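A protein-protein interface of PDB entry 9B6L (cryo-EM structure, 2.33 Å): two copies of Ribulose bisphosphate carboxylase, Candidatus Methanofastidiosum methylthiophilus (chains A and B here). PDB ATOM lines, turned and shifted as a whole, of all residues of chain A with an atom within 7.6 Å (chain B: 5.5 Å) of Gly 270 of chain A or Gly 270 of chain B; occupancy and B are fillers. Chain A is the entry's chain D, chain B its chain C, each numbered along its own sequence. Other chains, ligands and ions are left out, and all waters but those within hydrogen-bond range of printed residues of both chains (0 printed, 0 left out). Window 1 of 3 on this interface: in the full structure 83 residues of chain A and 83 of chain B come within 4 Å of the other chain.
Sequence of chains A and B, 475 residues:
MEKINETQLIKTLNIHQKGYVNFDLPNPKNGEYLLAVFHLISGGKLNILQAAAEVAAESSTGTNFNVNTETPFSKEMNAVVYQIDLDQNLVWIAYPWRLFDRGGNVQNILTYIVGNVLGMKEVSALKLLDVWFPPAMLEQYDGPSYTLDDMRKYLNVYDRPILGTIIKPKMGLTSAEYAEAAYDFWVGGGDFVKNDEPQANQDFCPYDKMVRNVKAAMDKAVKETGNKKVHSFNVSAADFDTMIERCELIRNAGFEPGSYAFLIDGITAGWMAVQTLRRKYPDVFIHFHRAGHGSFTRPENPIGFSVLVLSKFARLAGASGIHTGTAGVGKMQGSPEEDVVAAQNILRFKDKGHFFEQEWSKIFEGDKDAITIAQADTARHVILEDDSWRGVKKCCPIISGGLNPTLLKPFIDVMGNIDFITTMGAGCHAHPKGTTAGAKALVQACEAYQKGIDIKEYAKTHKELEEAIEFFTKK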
ATOM      1  N   GLN A 107      12.194  28.504   2.814  1.00  0.00           N
ATOM      2  CA  GLN A 107      11.581  28.962   1.574  1.00  0.00           C
ATOM      3  C   GLN A 107      10.816  30.262   1.777  1.00  0.00           C
ATOM      4  O   GLN A 107      10.683  31.044   0.838  1.00  0.00           O
ATOM      5  CB  GLN A 107      10.683  27.864   0.981  1.00  0.00           C
ATOM      6  CG  GLN A 107       9.281  27.719   1.576  1.00  0.00           C
ATOM      7  CD  GLN A 107       8.290  28.760   1.090  1.00  0.00           C
ATOM      8  OE1 GLN A 107       8.386  29.256  -0.030  1.00  0.00           O
ATOM      9  NE2 GLN A 107       7.358  29.126   1.954  1.00  0.00           N
ATOM     10  N   SER A 236      14.470  12.620  -4.717  1.00  0.00           N
ATOM     11  CA  SER A 236      13.615  13.615  -5.351  1.00  0.00           C
ATOM     12  C   SER A 236      12.533  12.922  -6.169  1.00  0.00           C
ATOM     13  O   SER A 236      12.831  12.087  -7.028  1.00  0.00           O
ATOM     14  CB  SER A 236      14.449  14.539  -6.234  1.00  0.00           C
ATOM     15  OG  SER A 236      15.690  14.841  -5.625  1.00  0.00           O
ATOM     16  N   ALA A 238       7.999  13.051  -7.480  1.00  0.00           N
ATOM     17  CA  ALA A 238       6.913  13.917  -7.924  1.00  0.00           C
ATOM     18  C   ALA A 238       6.279  14.654  -6.753  1.00  0.00           C
ATOM     19  O   ALA A 238       6.064  15.869  -6.817  1.00  0.00           O
ATOM     20  CB  ALA A 238       5.861  13.099  -8.669  1.00  0.00           C
ATOM     21  N   PHE A 240       5.571  14.547  -2.109  1.00  0.00           N
ATOM     22  CA  PHE A 240       6.212  14.201  -0.846  1.00  0.00           C
ATOM     23  C   PHE A 240       5.940  12.752  -0.467  1.00  0.00           C
ATOM     24  O   PHE A 240       6.789  12.094   0.145  1.00  0.00           O
ATOM     25  CB  PHE A 240       5.744  15.153   0.255  1.00  0.00           C
ATOM     26  CG  PHE A 240       6.333  16.530   0.145  1.00  0.00           C
ATOM     27  CD1 PHE A 240       7.657  16.760   0.472  1.00  0.00           C
ATOM     28  CD2 PHE A 240       5.566  17.596  -0.293  1.00  0.00           C
ATOM     29  CE1 PHE A 240       8.201  18.021   0.365  1.00  0.00           C
ATOM     30  CE2 PHE A 240       6.107  18.859  -0.402  1.00  0.00           C
ATOM     31  CZ  PHE A 240       7.426  19.071  -0.073  1.00  0.00           C
ATOM     32  N   MET A 243       8.504  10.630  -2.348  1.00  0.00           N
ATOM     33  CA  MET A 243       9.823  10.802  -1.748  1.00  0.00           C
ATOM     34  C   MET A 243       9.937  10.041  -0.434  1.00  0.00           C
ATOM     35  O   MET A 243      10.945   9.372  -0.178  1.00  0.00           O
ATOM     36  CB  MET A 243      10.111  12.286  -1.540  1.00  0.00           C
ATOM     37  CG  MET A 243      11.157  12.589  -0.482  1.00  0.00           C
ATOM     38  SD  MET A 243      11.608  14.331  -0.456  1.00  0.00           S
ATOM     39  CE  MET A 243      11.086  14.777   1.194  1.00  0.00           C
ATOM     40  N   ILE A 264      18.786  15.079  -2.587  1.00  0.00           N
ATOM     41  CA  ILE A 264      17.615  15.865  -2.947  1.00  0.00           C
ATOM     42  C   ILE A 264      18.038  16.947  -3.928  1.00  0.00           C
ATOM     43  O   ILE A 264      19.074  17.597  -3.745  1.00  0.00           O
ATOM     44  CB  ILE A 264      16.935  16.474  -1.700  1.00  0.00           C
ATOM     45  CG1 ILE A 264      15.662  17.226  -2.089  1.00  0.00           C
ATOM     46  CG2 ILE A 264      17.902  17.352  -0.909  1.00  0.00           C
ATOM     47  CD1 ILE A 264      14.557  16.324  -2.585  1.00  0.00           C
ATOM     48  N   ASP A 265      17.254  17.119  -4.987  1.00  0.00           N
ATOM     49  CA  ASP A 265      17.443  18.236  -5.910  1.00  0.00           C
ATOM     50  C   ASP A 265      16.854  19.468  -5.239  1.00  0.00           C
ATOM     51  O   ASP A 265      15.657  19.732  -5.314  1.00  0.00           O
ATOM     52  CB  ASP A 265      16.782  17.955  -7.253  1.00  0.00           C
ATOM     53  CG  ASP A 265      17.324  16.708  -7.921  1.00  0.00           C
ATOM     54  OD1 ASP A 265      18.556  16.516  -7.919  1.00  0.00           O
ATOM     55  OD2 ASP A 265      16.518  15.922  -8.450  1.00  0.00           O
ATOM     56  N   GLY A 266      17.713  20.232  -4.564  1.00  0.00           N
ATOM     57  CA  GLY A 266      17.224  21.317  -3.732  1.00  0.00           C
ATOM     58  C   GLY A 266      16.509  22.407  -4.502  1.00  0.00           C
ATOM     59  O   GLY A 266      15.552  22.999  -4.002  1.00  0.00           O
ATOM     60  N   ILE A 267      16.956  22.688  -5.724  1.00  0.00           N
ATOM     61  CA  ILE A 267      16.372  23.777  -6.498  1.00  0.00           C
ATOM     62  C   ILE A 267      15.073  23.335  -7.165  1.00  0.00           C
ATOM     63  O   ILE A 267      14.029  23.976  -7.009  1.00  0.00           O
ATOM     64  CB  ILE A 267      17.387  24.304  -7.529  1.00  0.00           C
ATOM     65  CG1 ILE A 267      18.692  24.698  -6.834  1.00  0.00           C
ATOM     66  CG2 ILE A 267      16.807  25.477  -8.303  1.00  0.00           C
ATOM     67  CD1 ILE A 267      18.527  25.738  -5.749  1.00  0.00           C
ATOM     68  N   THR A 268      15.119  22.236  -7.924  1.00  0.00           N
ATOM     69  CA  THR A 268      13.933  21.813  -8.666  1.00  0.00           C
ATOM     70  C   THR A 268      12.884  21.204  -7.741  1.00  0.00           C
ATOM     71  O   THR A 268      11.705  21.572  -7.801  1.00  0.00           O
ATOM     72  CB  THR A 268      14.317  20.828  -9.773  1.00  0.00           C
ATOM     73  OG1 THR A 268      14.917  19.660  -9.201  1.00  0.00           O
ATOM     74  CG2 THR A 268      15.291  21.471 -10.747  1.00  0.00           C
ATOM     75  N   ALA A 269      13.290  20.277  -6.870  1.00  0.00           N
ATOM     76  CA  ALA A 269      12.327  19.661  -5.962  1.00  0.00           C
ATOM     77  C   ALA A 269      11.856  20.641  -4.896  1.00  0.00           C
ATOM     78  O   ALA A 269      10.699  20.576  -4.468  1.00  0.00           O
ATOM     79  CB  ALA A 269      12.920  18.409  -5.319  1.00  0.00           C
ATOM     80  N   GLY A 270      12.720  21.542  -4.459  1.00  0.00           N
ATOM     81  CA  GLY A 270      12.306  22.638  -3.612  1.00  0.00           C
ATOM     82  C   GLY A 270      12.884  22.542  -2.209  1.00  0.00           C
ATOM     83  O   GLY A 270      13.277  21.477  -1.728  1.00  0.00           O
ATOM     84  N   TRP A 271      12.916  23.701  -1.547  1.00  0.00           N
ATOM     85  CA  TRP A 271      13.434  23.790  -0.187  1.00  0.00           C
ATOM     86  C   TRP A 271      12.543  23.059   0.804  1.00  0.00           C
ATOM     87  O   TRP A 271      13.014  22.626   1.864  1.00  0.00           O
ATOM     88  CB  TRP A 271      13.584  25.258   0.200  1.00  0.00           C
ATOM     89  CG  TRP A 271      14.645  25.934  -0.591  1.00  0.00           C
ATOM     90  CD1 TRP A 271      14.490  26.595  -1.771  1.00  0.00           C
ATOM     91  CD2 TRP A 271      16.034  26.004  -0.269  1.00  0.00           C
ATOM     92  NE1 TRP A 271      15.699  27.073  -2.205  1.00  0.00           N
ATOM     93  CE2 TRP A 271      16.665  26.722  -1.301  1.00  0.00           C
ATOM     94  CE3 TRP A 271      16.808  25.529   0.791  1.00  0.00           C
ATOM     95  CZ2 TRP A 271      18.028  26.986  -1.296  1.00  0.00           C
ATOM     96  CZ3 TRP A 271      18.157  25.786   0.790  1.00  0.00           C
ATOM     97  CH2 TRP A 271      18.756  26.509  -0.245  1.00  0.00           C
ATOM     98  N   MET A 272      11.259  22.916   0.479  1.00  0.00           N
ATOM     99  CA  MET A 272      10.355  22.185   1.354  1.00  0.00           C
ATOM    100  C   MET A 272      10.750  20.721   1.450  1.00  0.00           C
ATOM    101  O   MET A 272      10.686  20.125   2.528  1.00  0.00           O
ATOM    102  CB  MET A 272       8.924  22.329   0.855  1.00  0.00           C
ATOM    103  CG  MET A 272       8.178  23.440   1.537  1.00  0.00           C
ATOM    104  SD  MET A 272       6.537  23.667   0.860  1.00  0.00           S
ATOM    105  CE  MET A 272       5.663  22.499   1.878  1.00  0.00           C
ATOM    106  N   ALA A 273      11.159  20.123   0.329  1.00  0.00           N
ATOM    107  CA  ALA A 273      11.628  18.744   0.354  1.00  0.00           C
ATOM    108  C   ALA A 273      12.901  18.609   1.178  1.00  0.00           C
ATOM    109  O   ALA A 273      13.067  17.636   1.920  1.00  0.00           O
ATOM    110  CB  ALA A 273      11.850  18.236  -1.070  1.00  0.00           C
ATOM    111  N   VAL A 274      13.813  19.576   1.059  1.00  0.00           N
ATOM    112  CA  VAL A 274      15.046  19.537   1.841  1.00  0.00           C
ATOM    113  C   VAL A 274      14.732  19.584   3.330  1.00  0.00           C
ATOM    114  O   VAL A 274      15.258  18.791   4.121  1.00  0.00           O
ATOM    115  CB  VAL A 274      15.982  20.687   1.426  1.00  0.00           C
ATOM    116  CG1 VAL A 274      17.214  20.711   2.315  1.00  0.00           C
ATOM    117  CG2 VAL A 274      16.373  20.552  -0.034  1.00  0.00           C
ATOM    118  N   GLN A 275      13.855  20.508   3.735  1.00  0.00           N
ATOM    119  CA  GLN A 275      13.498  20.610   5.146  1.00  0.00           C
ATOM    120  C   GLN A 275      12.753  19.369   5.626  1.00  0.00           C
ATOM    121  O   GLN A 275      12.961  18.915   6.758  1.00  0.00           O
ATOM    122  CB  GLN A 275      12.672  21.870   5.393  1.00  0.00           C
ATOM    123  CG  GLN A 275      13.440  23.159   5.154  1.00  0.00           C
ATOM    124  CD  GLN A 275      12.824  24.350   5.858  1.00  0.00           C
ATOM    125  OE1 GLN A 275      12.360  25.290   5.216  1.00  0.00           O
ATOM    126  NE2 GLN A 275      12.818  24.318   7.183  1.00  0.00           N
ATOM    127  N   THR A 276      11.878  18.810   4.786  1.00  0.00           N
ATOM    128  CA  THR A 276      11.166  17.592   5.155  1.00  0.00           C
ATOM    129  C   THR A 276      12.128  16.430   5.359  1.00  0.00           C
ATOM    130  O   THR A 276      11.982  15.658   6.311  1.00  0.00           O
ATOM    131  CB  THR A 276      10.124  17.250   4.087  1.00  0.00           C
ATOM    132  OG1 THR A 276       9.283  18.385   3.856  1.00  0.00           O
ATOM    133  CG2 THR A 276       9.270  16.073   4.529  1.00  0.00           C
ATOM    134  N   PHE A 288      22.384  17.700  -0.591  1.00  0.00           N
ATOM    135  CA  PHE A 288      21.734  18.774  -1.333  1.00  0.00           C
ATOM    136  C   PHE A 288      22.379  18.875  -2.710  1.00  0.00           C
ATOM    137  O   PHE A 288      23.517  19.336  -2.837  1.00  0.00           O
ATOM    138  CB  PHE A 288      21.846  20.092  -0.568  1.00  0.00           C
ATOM    139  CG  PHE A 288      21.010  21.217  -1.131  1.00  0.00           C
ATOM    140  CD1 PHE A 288      21.302  21.782  -2.364  1.00  0.00           C
ATOM    141  CD2 PHE A 288      19.945  21.728  -0.408  1.00  0.00           C
ATOM    142  CE1 PHE A 288      20.542  22.817  -2.868  1.00  0.00           C
ATOM    143  CE2 PHE A 288      19.184  22.767  -0.910  1.00  0.00           C
ATOM    144  CZ  PHE A 288      19.483  23.312  -2.137  1.00  0.00           C
ATOM    145  N   ILE B 264       0.601  28.423  -3.414  1.00  0.00           N
ATOM    146  CA  ILE B 264       1.900  27.805  -3.203  1.00  0.00           C
ATOM    147  C   ILE B 264       2.957  28.631  -3.919  1.00  0.00           C
ATOM    148  O   ILE B 264       2.757  29.061  -5.062  1.00  0.00           O
ATOM    149  CB  ILE B 264       1.915  26.337  -3.688  1.00  0.00           C
ATOM    150  CG1 ILE B 264       3.262  25.676  -3.383  1.00  0.00           C
ATOM    151  CG2 ILE B 264       1.545  26.233  -5.166  1.00  0.00           C
ATOM    152  CD1 ILE B 264       3.514  25.475  -1.909  1.00  0.00           C
ATOM    153  N   ASP B 265       4.069  28.885  -3.236  1.00  0.00           N
ATOM    154  CA  ASP B 265       5.229  29.511  -3.863  1.00  0.00           C
ATOM    155  C   ASP B 265       5.935  28.429  -4.668  1.00  0.00           C
ATOM    156  O   ASP B 265       6.747  27.667  -4.148  1.00  0.00           O
ATOM    157  CB  ASP B 265       6.149  30.129  -2.819  1.00  0.00           C
ATOM    158  CG  ASP B 265       5.457  31.179  -1.977  1.00  0.00           C
ATOM    159  OD1 ASP B 265       4.718  32.006  -2.544  1.00  0.00           O
ATOM    160  OD2 ASP B 265       5.654  31.179  -0.747  1.00  0.00           O
ATOM    161  N   GLY B 266       5.615  28.360  -5.958  1.00  0.00           N
ATOM    162  CA  GLY B 266       6.082  27.248  -6.766  1.00  0.00           C
ATOM    163  C   GLY B 266       7.588  27.180  -6.905  1.00  0.00           C
ATOM    164  O   GLY B 266       8.161  26.090  -6.963  1.00  0.00           O
ATOM    165  N   ILE B 267       8.251  28.332  -6.958  1.00  0.00           N
ATOM    166  CA  ILE B 267       9.695  28.353  -7.167  1.00  0.00           C
ATOM    167  C   ILE B 267      10.437  28.079  -5.864  1.00  0.00           C
ATOM    168  O   ILE B 267      11.283  27.181  -5.791  1.00  0.00           O
ATOM    169  CB  ILE B 267      10.124  29.691  -7.793  1.00  0.00           C
ATOM    170  CG1 ILE B 267       9.329  29.957  -9.073  1.00  0.00           C
ATOM    171  CG2 ILE B 267      11.619  29.699  -8.070  1.00  0.00           C
ATOM    172  CD1 ILE B 267       9.460  28.873 -10.121  1.00  0.00           C
ATOM    173  N   THR B 268      10.142  28.853  -4.816  1.00  0.00           N
ATOM    174  CA  THR B 268      10.883  28.705  -3.566  1.00  0.00           C
ATOM    175  C   THR B 268      10.479  27.435  -2.823  1.00  0.00           C
ATOM    176  O   THR B 268      11.339  26.657  -2.396  1.00  0.00           O
ATOM    177  CB  THR B 268      10.691  29.936  -2.679  1.00  0.00           C
ATOM    178  OG1 THR B 268       9.306  30.091  -2.349  1.00  0.00           O
ATOM    179  CG2 THR B 268      11.183  31.188  -3.389  1.00  0.00           C
ATOM    180  N   ALA B 269       9.173  27.202  -2.664  1.00  0.00           N
ATOM    181  CA  ALA B 269       8.731  26.002  -1.957  1.00  0.00           C
ATOM    182  C   ALA B 269       8.988  24.743  -2.775  1.00  0.00           C
ATOM    183  O   ALA B 269       9.276  23.686  -2.206  1.00  0.00           O
ATOM    184  CB  ALA B 269       7.254  26.111  -1.587  1.00  0.00           C
ATOM    185  N   GLY B 270       8.892  24.832  -4.092  1.00  0.00           N
ATOM    186  CA  GLY B 270       9.322  23.754  -4.955  1.00  0.00           C
ATOM    187  C   GLY B 270       8.164  23.100  -5.692  1.00  0.00           C
ATOM    188  O   GLY B 270       7.000  23.174  -5.291  1.00  0.00           O
ATOM    189  N   TRP B 271       8.517  22.437  -6.795  1.00  0.00           N
ATOM    190  CA  TRP B 271       7.533  21.749  -7.622  1.00  0.00           C
ATOM    191  C   TRP B 271       6.931  20.552  -6.903  1.00  0.00           C
ATOM    192  O   TRP B 271       5.805  20.140  -7.214  1.00  0.00           O
ATOM    193  CB  TRP B 271       8.185  21.321  -8.933  1.00  0.00           C
ATOM    194  CG  TRP B 271       8.552  22.487  -9.777  1.00  0.00           C
ATOM    195  CD1 TRP B 271       9.736  23.157  -9.780  1.00  0.00           C
ATOM    196  CD2 TRP B 271       7.720  23.137 -10.741  1.00  0.00           C
ATOM    197  NE1 TRP B 271       9.696  24.186 -10.684  1.00  0.00           N
ATOM    198  CE2 TRP B 271       8.466  24.197 -11.287  1.00  0.00           C
ATOM    199  CE3 TRP B 271       6.416  22.927 -11.193  1.00  0.00           C
ATOM    200  CZ2 TRP B 271       7.956  25.035 -12.270  1.00  0.00           C
ATOM    201  CZ3 TRP B 271       5.913  23.762 -12.161  1.00  0.00           C
ATOM    202  CH2 TRP B 271       6.679  24.802 -12.691  1.00  0.00           C
ATOM    203  N   MET B 272       7.663  19.985  -5.945  1.00  0.00           N
ATOM    204  CA  MET B 272       7.133  18.865  -5.183  1.00  0.00           C
ATOM    205  C   MET B 272       5.929  19.285  -4.355  1.00  0.00           C
ATOM    206  O   MET B 272       4.952  18.539  -4.250  1.00  0.00           O
ATOM    207  CB  MET B 272       8.220  18.282  -4.291  1.00  0.00           C
ATOM    208  CG  MET B 272       8.908  17.101  -4.909  1.00  0.00           C
ATOM    209  SD  MET B 272      10.280  16.516  -3.917  1.00  0.00           S
ATOM    210  CE  MET B 272       9.384  15.374  -2.887  1.00  0.00           C
ATOM    211  N   ALA B 273       5.984  20.478  -3.760  1.00  0.00           N
ATOM    212  CA  ALA B 273       4.840  20.984  -3.012  1.00  0.00           C
ATOM    213  C   ALA B 273       3.647  21.224  -3.927  1.00  0.00           C
ATOM    214  O   ALA B 273       2.504  20.939  -3.552  1.00  0.00           O
ATOM    215  CB  ALA B 273       5.220  22.267  -2.273  1.00  0.00           C
ATOM    216  N   VAL B 274       3.891  21.750  -5.129  1.00  0.00           N
ATOM    217  CA  VAL B 274       2.803  21.979  -6.076  1.00  0.00           C
ATOM    218  C   VAL B 274       2.131  20.661  -6.442  1.00  0.00           C
ATOM    219  O   VAL B 274       0.899  20.545  -6.422  1.00  0.00           O
ATOM    220  CB  VAL B 274       3.324  22.712  -7.326  1.00  0.00           C
ATOM    221  CG1 VAL B 274       2.216  22.844  -8.361  1.00  0.00           C
ATOM    222  CG2 VAL B 274       3.878  24.075  -6.952  1.00  0.00           C
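OE1 of Gln 107 of chain A lies close to OD2 of Asp 265 of chain B (3.4 Å).
The side-chain hydroxyl (OG1) of Thr 268 of chain B sits at hydrogen-bond distance from the side-chain amide oxygen (OE1) of Gln 107 of chain A, at 2.6 Å.
The backbone carbonyl oxygen (O) of Thr 268 of chain B lies close to the backbone NH (N) of Trp 271 of chain A, 3.5 Å away.
N of Ala 269 of chain B sits at hydrogen-bond distance from OE1 of Gln 107 of chain A, 3.4 Å away.
N of Met 272 of chain A sits close to O of Ala 269 of chain B (3.4 Å).
The backbone NH (N) of Trp 271 of chain B lies close to the backbone carbonyl oxygen (O) of Thr 268 of chain A (3.5 Å).
N of Met 272 of chain B sits close to O of Ala 269 of chain A (3.4 Å).
The side-chain hydroxyl (OG1) of Thr 276 of chain A is in hydrogen-bond range of the backbone carbonyl oxygen (O) of Met 272 of chain A (2.6 Å).
CA of Phe 240 of chain A touches CE of Met 272 of chain B, at 3.95 Å.
Phe 240 of chain A touches Ala 273 of chain B.
Met 272 of chain B touches Met 243 of chain A.
Ala 269 of chain A touches Gly 270 of chain B (O to CA, 3.5 Å).
Ala 269 of chain A touches Trp 271 of chain B (O to N, 3.7 Å).
Gly 270 of chain A touches Ala 269 of chain B (CA to O, 3.5 Å).
Gly 270 of chain B touches Gly 270 of chain A (CA to CA, 3.5 Å).
O of Ala 269 of chain B touches N of Trp 271 of chain A, at 3.7 Å.
Ala 273 of chain B touches Met 272 of chain A (CB to SD, 3.7 Å).
Ala 273 of chain A touches Met 272 of chain B (CB to SD, 3.7 Å).
Of the printed residues of chain B, Gln 107 of chain A touches Asp 265 (3.4 Å), Thr 268 (2.6 Å) and Ala 269 (3.4 Å).
Of the printed residues of chain B, Ala 238 of chain A touches Met 272 (3.6 Å).
Of the printed residues of chain B, Ala 269 of chain A touches Gly 270 (3.5 Å), Trp 271 (3.7 Å) and Met 272 (3.4 Å).
Of the printed residues of chain B, Gly 270 of chain A touches Ala 269 (3.5 Å) and Gly 270 (3.5 Å).
Of chain A, only Gln 107 (3.4 Å), Gly 270 (3.5 Å), Trp 271 (3.7 Å) and Met 272 (3.4 Å) come within 4 Å of Ala 269 of chain B.
Of chain A, only Ala 269 and Gly 270 come within 4 Å of Gly 270 of chain B.
The nearest residue of chain B that does not touch Gly 270 of chain A is Thr 268 of chain B (4.3 Å).
The nearest residue of chain A that does not touch Gly 270 of chain B is Thr 268 of chain A (4.3 Å).
Printed residues of chain B that touch a printed residue of chain A: Asp 265, Thr 268, Ala 269, Gly 270, Trp 271, Met 272 and Ala 273.
Of the 19 printed residues of chain A, 10 touch a printed residue of chain B.
Printed residues of chain A that touch a printed residue of chain B: Gln 107, Ala 238, Phe 240, Met 243, Thr 268, Ala 269, Gly 270, Trp 271, Met 272 and Ala 273.
Among the printed residues, no Asp or Glu carboxylate lies within 4 Å of a Lys or Arg side-chain nitrogen of the other chain.
Thr 268 of chain A touches Trp 271 of chain B, and with the chains exchanged Trp 271 of chain A touches Thr 268 of chain B.
Ala 269 of chain A touches Gly 270 of chain B, and with the chains exchanged Gly 270 of chain A touches Ala 269 of chain B.
Gly 270 of chain A touches its own counterpart, Gly 270 of chain B.
Met 272 of chain A touches Ala 273 of chain B, and with the chains exchanged Ala 273 of chain A touches Met 272 of chain B.
11 positions are printed for both chains.
Of the 18 pairs that touch across the chains among the printed residues, 11 have their exchanged pair printed and touching as well.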
